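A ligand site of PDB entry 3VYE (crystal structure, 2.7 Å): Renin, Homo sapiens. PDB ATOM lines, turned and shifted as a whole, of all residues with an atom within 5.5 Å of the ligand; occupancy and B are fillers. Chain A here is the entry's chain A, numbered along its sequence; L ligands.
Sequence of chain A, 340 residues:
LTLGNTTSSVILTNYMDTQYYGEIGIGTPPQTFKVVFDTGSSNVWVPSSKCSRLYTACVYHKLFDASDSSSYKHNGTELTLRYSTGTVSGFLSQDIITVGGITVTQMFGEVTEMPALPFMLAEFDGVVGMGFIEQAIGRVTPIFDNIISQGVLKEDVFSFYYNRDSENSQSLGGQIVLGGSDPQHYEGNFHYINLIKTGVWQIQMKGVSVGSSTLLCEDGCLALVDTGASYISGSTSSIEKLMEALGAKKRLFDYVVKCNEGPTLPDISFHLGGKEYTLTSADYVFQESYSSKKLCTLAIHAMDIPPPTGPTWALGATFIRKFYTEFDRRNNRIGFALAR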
ATOM      1  N   THR A  18     -12.845  31.917  34.547  1.00  0.00           N
ATOM      2  CA  THR A  18     -13.089  30.472  34.547  1.00  0.00           C
ATOM      3  C   THR A  18     -13.311  29.866  33.160  1.00  0.00           C
ATOM      4  O   THR A  18     -13.158  28.660  32.992  1.00  0.00           O
ATOM      5  CB  THR A  18     -14.309  30.096  35.384  1.00  0.00           C
ATOM      6  OG1 THR A  18     -15.498  30.583  34.758  1.00  0.00           O
ATOM      7  CG2 THR A  18     -14.188  30.664  36.745  1.00  0.00           C
ATOM      8  N   GLN A  19     -13.709  30.694  32.190  1.00  0.00           N
ATOM      9  CA  GLN A  19     -13.938  30.204  30.823  1.00  0.00           C
ATOM     10  C   GLN A  19     -13.294  31.126  29.789  1.00  0.00           C
ATOM     11  O   GLN A  19     -13.546  32.335  29.751  1.00  0.00           O
ATOM     12  CB  GLN A  19     -15.448  30.091  30.552  1.00  0.00           C
ATOM     13  CG  GLN A  19     -16.145  29.036  31.389  1.00  0.00           C
ATOM     14  CD  GLN A  19     -17.663  29.143  31.321  1.00  0.00           C
ATOM     15  OE1 GLN A  19     -18.238  29.233  30.245  1.00  0.00           O
ATOM     16  NE2 GLN A  19     -18.308  29.128  32.489  1.00  0.00           N
ATOM     17  N   VAL A  36     -14.388  26.475  23.551  1.00  0.00           N
ATOM     18  CA  VAL A  36     -13.269  26.440  24.478  1.00  0.00           C
ATOM     19  C   VAL A  36     -12.229  25.504  23.873  1.00  0.00           C
ATOM     20  O   VAL A  36     -12.577  24.461  23.326  1.00  0.00           O
ATOM     21  CB  VAL A  36     -13.736  25.886  25.857  1.00  0.00           C
ATOM     22  CG1 VAL A  36     -12.555  25.404  26.650  1.00  0.00           C
ATOM     23  CG2 VAL A  36     -14.462  26.962  26.637  1.00  0.00           C
ATOM     24  N   ASP A  38      -9.671  22.946  24.544  1.00  0.00           N
ATOM     25  CA  ASP A  38      -9.306  22.048  25.632  1.00  0.00           C
ATOM     26  C   ASP A  38      -8.202  21.038  25.352  1.00  0.00           C
ATOM     27  O   ASP A  38      -8.436  20.034  24.686  1.00  0.00           O
ATOM     28  CB  ASP A  38     -10.574  21.310  26.081  1.00  0.00           C
ATOM     29  CG  ASP A  38     -10.310  20.294  27.158  1.00  0.00           C
ATOM     30  OD1 ASP A  38      -9.432  20.531  28.008  1.00  0.00           O
ATOM     31  OD2 ASP A  38     -10.992  19.241  27.165  1.00  0.00           O
ATOM     32  N   GLY A  40      -7.289  19.102  27.220  1.00  0.00           N
ATOM     33  CA  GLY A  40      -7.669  17.938  27.991  1.00  0.00           C
ATOM     34  C   GLY A  40      -8.535  16.900  27.291  1.00  0.00           C
ATOM     35  O   GLY A  40      -8.860  15.880  27.893  1.00  0.00           O
ATOM     36  N   SER A  41      -8.911  17.153  26.049  1.00  0.00           N
ATOM     37  CA  SER A  41      -9.735  16.238  25.276  1.00  0.00           C
ATOM     38  C   SER A  41      -9.321  16.407  23.822  1.00  0.00           C
ATOM     39  O   SER A  41      -8.514  17.275  23.516  1.00  0.00           O
ATOM     40  CB  SER A  41     -11.224  16.561  25.468  1.00  0.00           C
ATOM     41  OG  SER A  41     -11.561  17.857  24.990  1.00  0.00           O
ATOM     42  N   SER A  42      -9.858  15.590  22.913  1.00  0.00           N
ATOM     43  CA  SER A  42      -9.467  15.677  21.519  1.00  0.00           C
ATOM     44  C   SER A  42     -10.590  15.721  20.493  1.00  0.00           C
ATOM     45  O   SER A  42     -10.356  15.534  19.300  1.00  0.00           O
ATOM     46  CB  SER A  42      -8.535  14.516  21.166  1.00  0.00           C
ATOM     47  OG  SER A  42      -7.512  14.382  22.122  1.00  0.00           O
ATOM     48  N   LEU A  81     -19.376  11.839  24.693  1.00  0.00           N
ATOM     49  CA  LEU A  81     -18.202  12.379  25.351  1.00  0.00           C
ATOM     50  C   LEU A  81     -18.460  12.514  26.834  1.00  0.00           C
ATOM     51  O   LEU A  81     -19.252  13.343  27.285  1.00  0.00           O
ATOM     52  CB  LEU A  81     -17.830  13.739  24.767  1.00  0.00           C
ATOM     53  CG  LEU A  81     -17.596  13.728  23.252  1.00  0.00           C
ATOM     54  CD1 LEU A  81     -17.442  15.178  22.772  1.00  0.00           C
ATOM     55  CD2 LEU A  81     -16.368  12.877  22.920  1.00  0.00           C
ATOM     56  N   ARG A  82     -17.777  11.677  27.602  1.00  0.00           N
ATOM     57  CA  ARG A  82     -17.934  11.699  29.032  1.00  0.00           C
ATOM     58  C   ARG A  82     -16.769  12.414  29.645  1.00  0.00           C
ATOM     59  O   ARG A  82     -15.667  11.865  29.718  1.00  0.00           O
ATOM     60  CB  ARG A  82     -18.008  10.284  29.577  1.00  0.00           C
ATOM     61  CG  ARG A  82     -19.076   9.440  28.934  1.00  0.00           C
ATOM     62  CD  ARG A  82     -19.025   8.016  29.458  1.00  0.00           C
ATOM     63  NE  ARG A  82     -20.000   7.131  28.811  1.00  0.00           N
ATOM     64  CZ  ARG A  82     -19.970   6.747  27.543  1.00  0.00           C
ATOM     65  NH1 ARG A  82     -19.002   7.180  26.728  1.00  0.00           N
ATOM     66  NH2 ARG A  82     -20.896   5.921  27.084  1.00  0.00           N
ATOM     67  N   TYR A  83     -17.011  13.652  30.055  1.00  0.00           N
ATOM     68  CA  TYR A  83     -15.983  14.474  30.667  1.00  0.00           C
ATOM     69  C   TYR A  83     -16.042  14.334  32.192  1.00  0.00           C
ATOM     70  O   TYR A  83     -16.966  13.736  32.752  1.00  0.00           O
ATOM     71  CB  TYR A  83     -16.162  15.938  30.297  1.00  0.00           C
ATOM     72  CG  TYR A  83     -16.060  16.271  28.825  1.00  0.00           C
ATOM     73  CD1 TYR A  83     -17.137  16.821  28.139  1.00  0.00           C
ATOM     74  CD2 TYR A  83     -14.854  16.091  28.138  1.00  0.00           C
ATOM     75  CE1 TYR A  83     -17.024  17.198  26.813  1.00  0.00           C
ATOM     76  CE2 TYR A  83     -14.737  16.467  26.803  1.00  0.00           C
ATOM     77  CZ  TYR A  83     -15.827  17.023  26.154  1.00  0.00           C
ATOM     78  OH  TYR A  83     -15.717  17.437  24.853  1.00  0.00           O
ATOM     79  N   SER A  84     -15.040  14.902  32.841  1.00  0.00           N
ATOM     80  CA  SER A  84     -14.886  14.884  34.287  1.00  0.00           C
ATOM     81  C   SER A  84     -16.083  15.481  35.030  1.00  0.00           C
ATOM     82  O   SER A  84     -16.415  15.046  36.133  1.00  0.00           O
ATOM     83  CB  SER A  84     -13.618  15.643  34.670  1.00  0.00           C
ATOM     84  OG  SER A  84     -13.689  16.984  34.198  1.00  0.00           O
ATOM     85  N   THR A  85     -16.724  16.487  34.439  1.00  0.00           N
ATOM     86  CA  THR A  85     -17.836  17.141  35.114  1.00  0.00           C
ATOM     87  C   THR A  85     -19.197  17.014  34.424  1.00  0.00           C
ATOM     88  O   THR A  85     -20.176  17.611  34.865  1.00  0.00           O
ATOM     89  CB  THR A  85     -17.552  18.642  35.299  1.00  0.00           C
ATOM     90  OG1 THR A  85     -17.357  19.254  34.011  1.00  0.00           O
ATOM     91  CG2 THR A  85     -16.305  18.850  36.139  1.00  0.00           C
ATOM     92  N   PRO A 118     -23.768  20.587  33.590  1.00  0.00           N
ATOM     93  CA  PRO A 118     -23.283  21.951  33.792  1.00  0.00           C
ATOM     94  C   PRO A 118     -23.421  22.910  32.618  1.00  0.00           C
ATOM     95  O   PRO A 118     -23.195  24.106  32.765  1.00  0.00           O
ATOM     96  CB  PRO A 118     -21.816  21.719  34.112  1.00  0.00           C
ATOM     97  CG  PRO A 118     -21.474  20.653  33.083  1.00  0.00           C
ATOM     98  CD  PRO A 118     -22.649  19.695  33.186  1.00  0.00           C
ATOM     99  N   PHE A 119     -23.792  22.406  31.452  1.00  0.00           N
ATOM    100  CA  PHE A 119     -23.859  23.236  30.261  1.00  0.00           C
ATOM    101  C   PHE A 119     -24.677  24.516  30.299  1.00  0.00           C
ATOM    102  O   PHE A 119     -24.439  25.419  29.497  1.00  0.00           O
ATOM    103  CB  PHE A 119     -24.233  22.344  29.068  1.00  0.00           C
ATOM    104  CG  PHE A 119     -23.212  21.243  28.840  1.00  0.00           C
ATOM    105  CD1 PHE A 119     -21.915  21.555  28.458  1.00  0.00           C
ATOM    106  CD2 PHE A 119     -23.524  19.933  29.157  1.00  0.00           C
ATOM    107  CE1 PHE A 119     -20.927  20.563  28.413  1.00  0.00           C
ATOM    108  CE2 PHE A 119     -22.535  18.941  29.113  1.00  0.00           C
ATOM    109  CZ  PHE A 119     -21.232  19.257  28.742  1.00  0.00           C
ATOM    110  N   LEU A 121     -24.423  26.566  32.536  1.00  0.00           N
ATOM    111  CA  LEU A 121     -23.465  27.511  33.091  1.00  0.00           C
ATOM    112  C   LEU A 121     -22.318  27.798  32.127  1.00  0.00           C
ATOM    113  O   LEU A 121     -21.356  28.455  32.501  1.00  0.00           O
ATOM    114  CB  LEU A 121     -22.893  26.991  34.415  1.00  0.00           C
ATOM    115  CG  LEU A 121     -23.861  26.834  35.586  1.00  0.00           C
ATOM    116  CD1 LEU A 121     -24.707  25.579  35.382  1.00  0.00           C
ATOM    117  CD2 LEU A 121     -23.101  26.712  36.880  1.00  0.00           C
ATOM    118  N   ALA A 122     -22.427  27.302  30.897  1.00  0.00           N
ATOM    119  CA  ALA A 122     -21.381  27.516  29.892  1.00  0.00           C
ATOM    120  C   ALA A 122     -21.658  28.747  29.039  1.00  0.00           C
ATOM    121  O   ALA A 122     -22.715  28.851  28.431  1.00  0.00           O
ATOM    122  CB  ALA A 122     -21.264  26.308  28.996  1.00  0.00           C
ATOM    123  N   PHE A 124     -19.715  29.412  26.561  1.00  0.00           N
ATOM    124  CA  PHE A 124     -19.354  28.854  25.253  1.00  0.00           C
ATOM    125  C   PHE A 124     -20.415  27.894  24.731  1.00  0.00           C
ATOM    126  O   PHE A 124     -21.227  27.396  25.492  1.00  0.00           O
ATOM    127  CB  PHE A 124     -18.015  28.116  25.365  1.00  0.00           C
ATOM    128  CG  PHE A 124     -18.023  26.976  26.363  1.00  0.00           C
ATOM    129  CD1 PHE A 124     -17.698  27.181  27.697  1.00  0.00           C
ATOM    130  CD2 PHE A 124     -18.366  25.687  25.959  1.00  0.00           C
ATOM    131  CE1 PHE A 124     -17.696  26.108  28.621  1.00  0.00           C
ATOM    132  CE2 PHE A 124     -18.378  24.617  26.856  1.00  0.00           C
ATOM    133  CZ  PHE A 124     -18.042  24.831  28.182  1.00  0.00           C
ATOM    134  N   VAL A 127     -16.731  22.771  22.362  1.00  0.00           N
ATOM    135  CA  VAL A 127     -15.364  22.535  22.766  1.00  0.00           C
ATOM    136  C   VAL A 127     -14.571  22.142  21.541  1.00  0.00           C
ATOM    137  O   VAL A 127     -15.090  21.521  20.624  1.00  0.00           O
ATOM    138  CB  VAL A 127     -15.269  21.373  23.791  1.00  0.00           C
ATOM    139  CG1 VAL A 127     -13.784  21.099  24.146  1.00  0.00           C
ATOM    140  CG2 VAL A 127     -16.123  21.694  25.052  1.00  0.00           C
ATOM    141  N   GLN A 135      -6.545  10.192  22.697  1.00  0.00           N
ATOM    142  CA  GLN A 135      -7.629  10.550  23.606  1.00  0.00           C
ATOM    143  C   GLN A 135      -8.933  10.855  22.878  1.00  0.00           C
ATOM    144  O   GLN A 135      -9.972  11.032  23.504  1.00  0.00           O
ATOM    145  CB  GLN A 135      -7.233  11.768  24.447  1.00  0.00           C
ATOM    146  CG  GLN A 135      -6.388  11.452  25.655  1.00  0.00           C
ATOM    147  CD  GLN A 135      -5.924  12.708  26.351  1.00  0.00           C
ATOM    148  OE1 GLN A 135      -5.925  12.786  27.578  1.00  0.00           O
ATOM    149  NE2 GLN A 135      -5.505  13.697  25.562  1.00  0.00           N
ATOM    150  N   ILE A 137     -12.307  10.364  20.886  1.00  0.00           N
ATOM    151  CA  ILE A 137     -13.306   9.323  20.988  1.00  0.00           C
ATOM    152  C   ILE A 137     -13.843   9.090  19.598  1.00  0.00           C
ATOM    153  O   ILE A 137     -13.947  10.037  18.813  1.00  0.00           O
ATOM    154  CB  ILE A 137     -14.438   9.721  21.959  1.00  0.00           C
ATOM    155  CG1 ILE A 137     -13.882   9.747  23.382  1.00  0.00           C
ATOM    156  CG2 ILE A 137     -15.624   8.739  21.870  1.00  0.00           C
ATOM    157  CD1 ILE A 137     -14.888  10.146  24.428  1.00  0.00           C
ATOM    158  N   ASP A 226      -3.902  21.245  31.549  1.00  0.00           N
ATOM    159  CA  ASP A 226      -5.243  21.384  30.978  1.00  0.00           C
ATOM    160  C   ASP A 226      -5.777  22.802  30.690  1.00  0.00           C
ATOM    161  O   ASP A 226      -6.219  23.501  31.613  1.00  0.00           O
ATOM    162  CB  ASP A 226      -6.195  20.653  31.927  1.00  0.00           C
ATOM    163  CG  ASP A 226      -7.520  20.350  31.303  1.00  0.00           C
ATOM    164  OD1 ASP A 226      -7.975  21.108  30.424  1.00  0.00           O
ATOM    165  OD2 ASP A 226      -8.132  19.336  31.722  1.00  0.00           O
ATOM    166  N   GLY A 228      -8.479  23.575  29.227  1.00  0.00           N
ATOM    167  CA  GLY A 228      -9.924  23.601  29.359  1.00  0.00           C
ATOM    168  C   GLY A 228     -10.422  23.562  30.794  1.00  0.00           C
ATOM    169  O   GLY A 228     -11.615  23.688  31.046  1.00  0.00           O
ATOM    170  N   ALA A 229      -9.492  23.382  31.737  1.00  0.00           N
ATOM    171  CA  ALA A 229      -9.814  23.331  33.159  1.00  0.00           C
ATOM    172  C   ALA A 229      -9.660  24.749  33.690  1.00  0.00           C
ATOM    173  O   ALA A 229      -8.721  25.455  33.330  1.00  0.00           O
ATOM    174  CB  ALA A 229      -8.851  22.383  33.879  1.00  0.00           C
ATOM    175  N   SER A 230     -10.582  25.177  34.545  1.00  0.00           N
ATOM    176  CA  SER A 230     -10.519  26.530  35.068  1.00  0.00           C
ATOM    177  C   SER A 230      -9.624  26.622  36.271  1.00  0.00           C
ATOM    178  O   SER A 230      -8.998  27.640  36.509  1.00  0.00           O
ATOM    179  CB  SER A 230     -11.900  27.024  35.500  1.00  0.00           C
ATOM    180  OG  SER A 230     -12.931  26.339  34.809  1.00  0.00           O
HETATM  181  C1  LIG L   1     -11.877  17.411  29.900  1.00  0.00           C
HETATM  182  C2  LIG L   1     -10.632  17.933  30.617  1.00  0.00           C
HETATM  183  N1  LIG L   1     -10.394  19.345  30.342  1.00  0.00           N
HETATM  184  C3  LIG L   1     -11.527  20.167  30.766  1.00  0.00           C
HETATM  185  C4  LIG L   1     -12.815  19.764  30.044  1.00  0.00           C
HETATM  186  C5  LIG L   1     -13.123  18.270  30.182  1.00  0.00           C
HETATM  187  N2  LIG L   1     -13.932  20.629  30.422  1.00  0.00           N
HETATM  188  C6  LIG L   1     -14.617  20.326  31.661  1.00  0.00           C
HETATM  189  C7  LIG L   1     -15.586  21.419  32.143  1.00  0.00           C
HETATM  190  N3  LIG L   1     -15.901  22.427  31.243  1.00  0.00           N
HETATM  191  C8  LIG L   1     -15.352  22.478  29.876  1.00  0.00           C
HETATM  192  C9  LIG L   1     -14.741  21.190  29.364  1.00  0.00           C
HETATM  193  O1  LIG L   1     -16.052  21.366  33.270  1.00  0.00           O
HETATM  194  C10 LIG L   1     -13.876  21.486  28.133  1.00  0.00           C
HETATM  195  C11 LIG L   1     -15.858  20.201  28.978  1.00  0.00           C
HETATM  196  C12 LIG L   1     -16.775  23.421  31.647  1.00  0.00           C
HETATM  197  C13 LIG L   1     -18.154  23.336  31.522  1.00  0.00           C
HETATM  198  C14 LIG L   1     -19.006  24.342  31.919  1.00  0.00           C
HETATM  199  C15 LIG L   1     -18.448  25.495  32.474  1.00  0.00           C
HETATM  200  C16 LIG L   1     -17.066  25.613  32.604  1.00  0.00           C
HETATM  201  C17 LIG L   1     -16.224  24.581  32.187  1.00  0.00           C
HETATM  202 CL1  LIG L   1     -18.835  21.904  30.849  1.00  0.00          CL
HETATM  203  C18 LIG L   1     -12.123  15.931  30.248  1.00  0.00           C
HETATM  204  O2  LIG L   1     -13.018  15.588  31.007  1.00  0.00           O
HETATM  205  N4  LIG L   1     -11.274  15.089  29.616  1.00  0.00           N
HETATM  206  C19 LIG L   1     -11.418  13.663  29.871  1.00  0.00           C
HETATM  207  C20 LIG L   1     -12.622  13.124  29.095  1.00  0.00           C
HETATM  208  C21 LIG L   1     -12.258  12.505  27.746  1.00  0.00           C
HETATM  209  C22 LIG L   1     -13.392  12.591  26.730  1.00  0.00           C
HETATM  210  C23 LIG L   1     -10.916  12.987  27.176  1.00  0.00           C
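The side-chain hydroxyl of Thr 85 lies within hydrogen-bond range of an oxygen (O1) of the ligand.
N1 of the ligand is in salt-bridge range of OD2 of Asp 226.
A nitrogen (N1) of the ligand is in salt-bridge range of the side-chain carboxylate of Asp 38 (2.8 Å).
O2 of the ligand is in hydrogen-bond range of N of Ser 84, at 2.8 Å.
The backbone carbonyl oxygen of Gly 40 sits at hydrogen-bond distance from a nitrogen (N4) of the ligand (3.1 Å).
N of Gly 228 sits at hydrogen-bond distance from OD1 of Asp 226.
N of Ala 229 sits at hydrogen-bond distance from OD1 of Asp 226 (3.0 Å).
OD1 of Asp 38 is in hydrogen-bond range of N of Gly 40 (2.7 Å).
The side-chain carboxylate (OD1) of Asp 38 lies close to the backbone NH (N) of Gly 228.
The side-chain carboxylate of Asp 38 sits at hydrogen-bond distance from the side-chain hydroxyl of Ser 41 (2.6 Å).
O of Leu 121 sits at hydrogen-bond distance from NE2 of Gln 19, 3.1 Å away.
Residues that only touch the ligand: Tyr 83, Arg 82, Phe 119, Gly 228, Gln 19, Phe 124, Ile 137, Pro 118, Val 127, Ala 229 and Ser 41.
Hydrophobic or aromatic side chains within 4 Å of the ligand: Tyr 83, Pro 118, Phe 119, Phe 124, Val 127 and Ile 137.
The nearest printed residue that does not touch the ligand is Leu 121 (4.1 Å).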
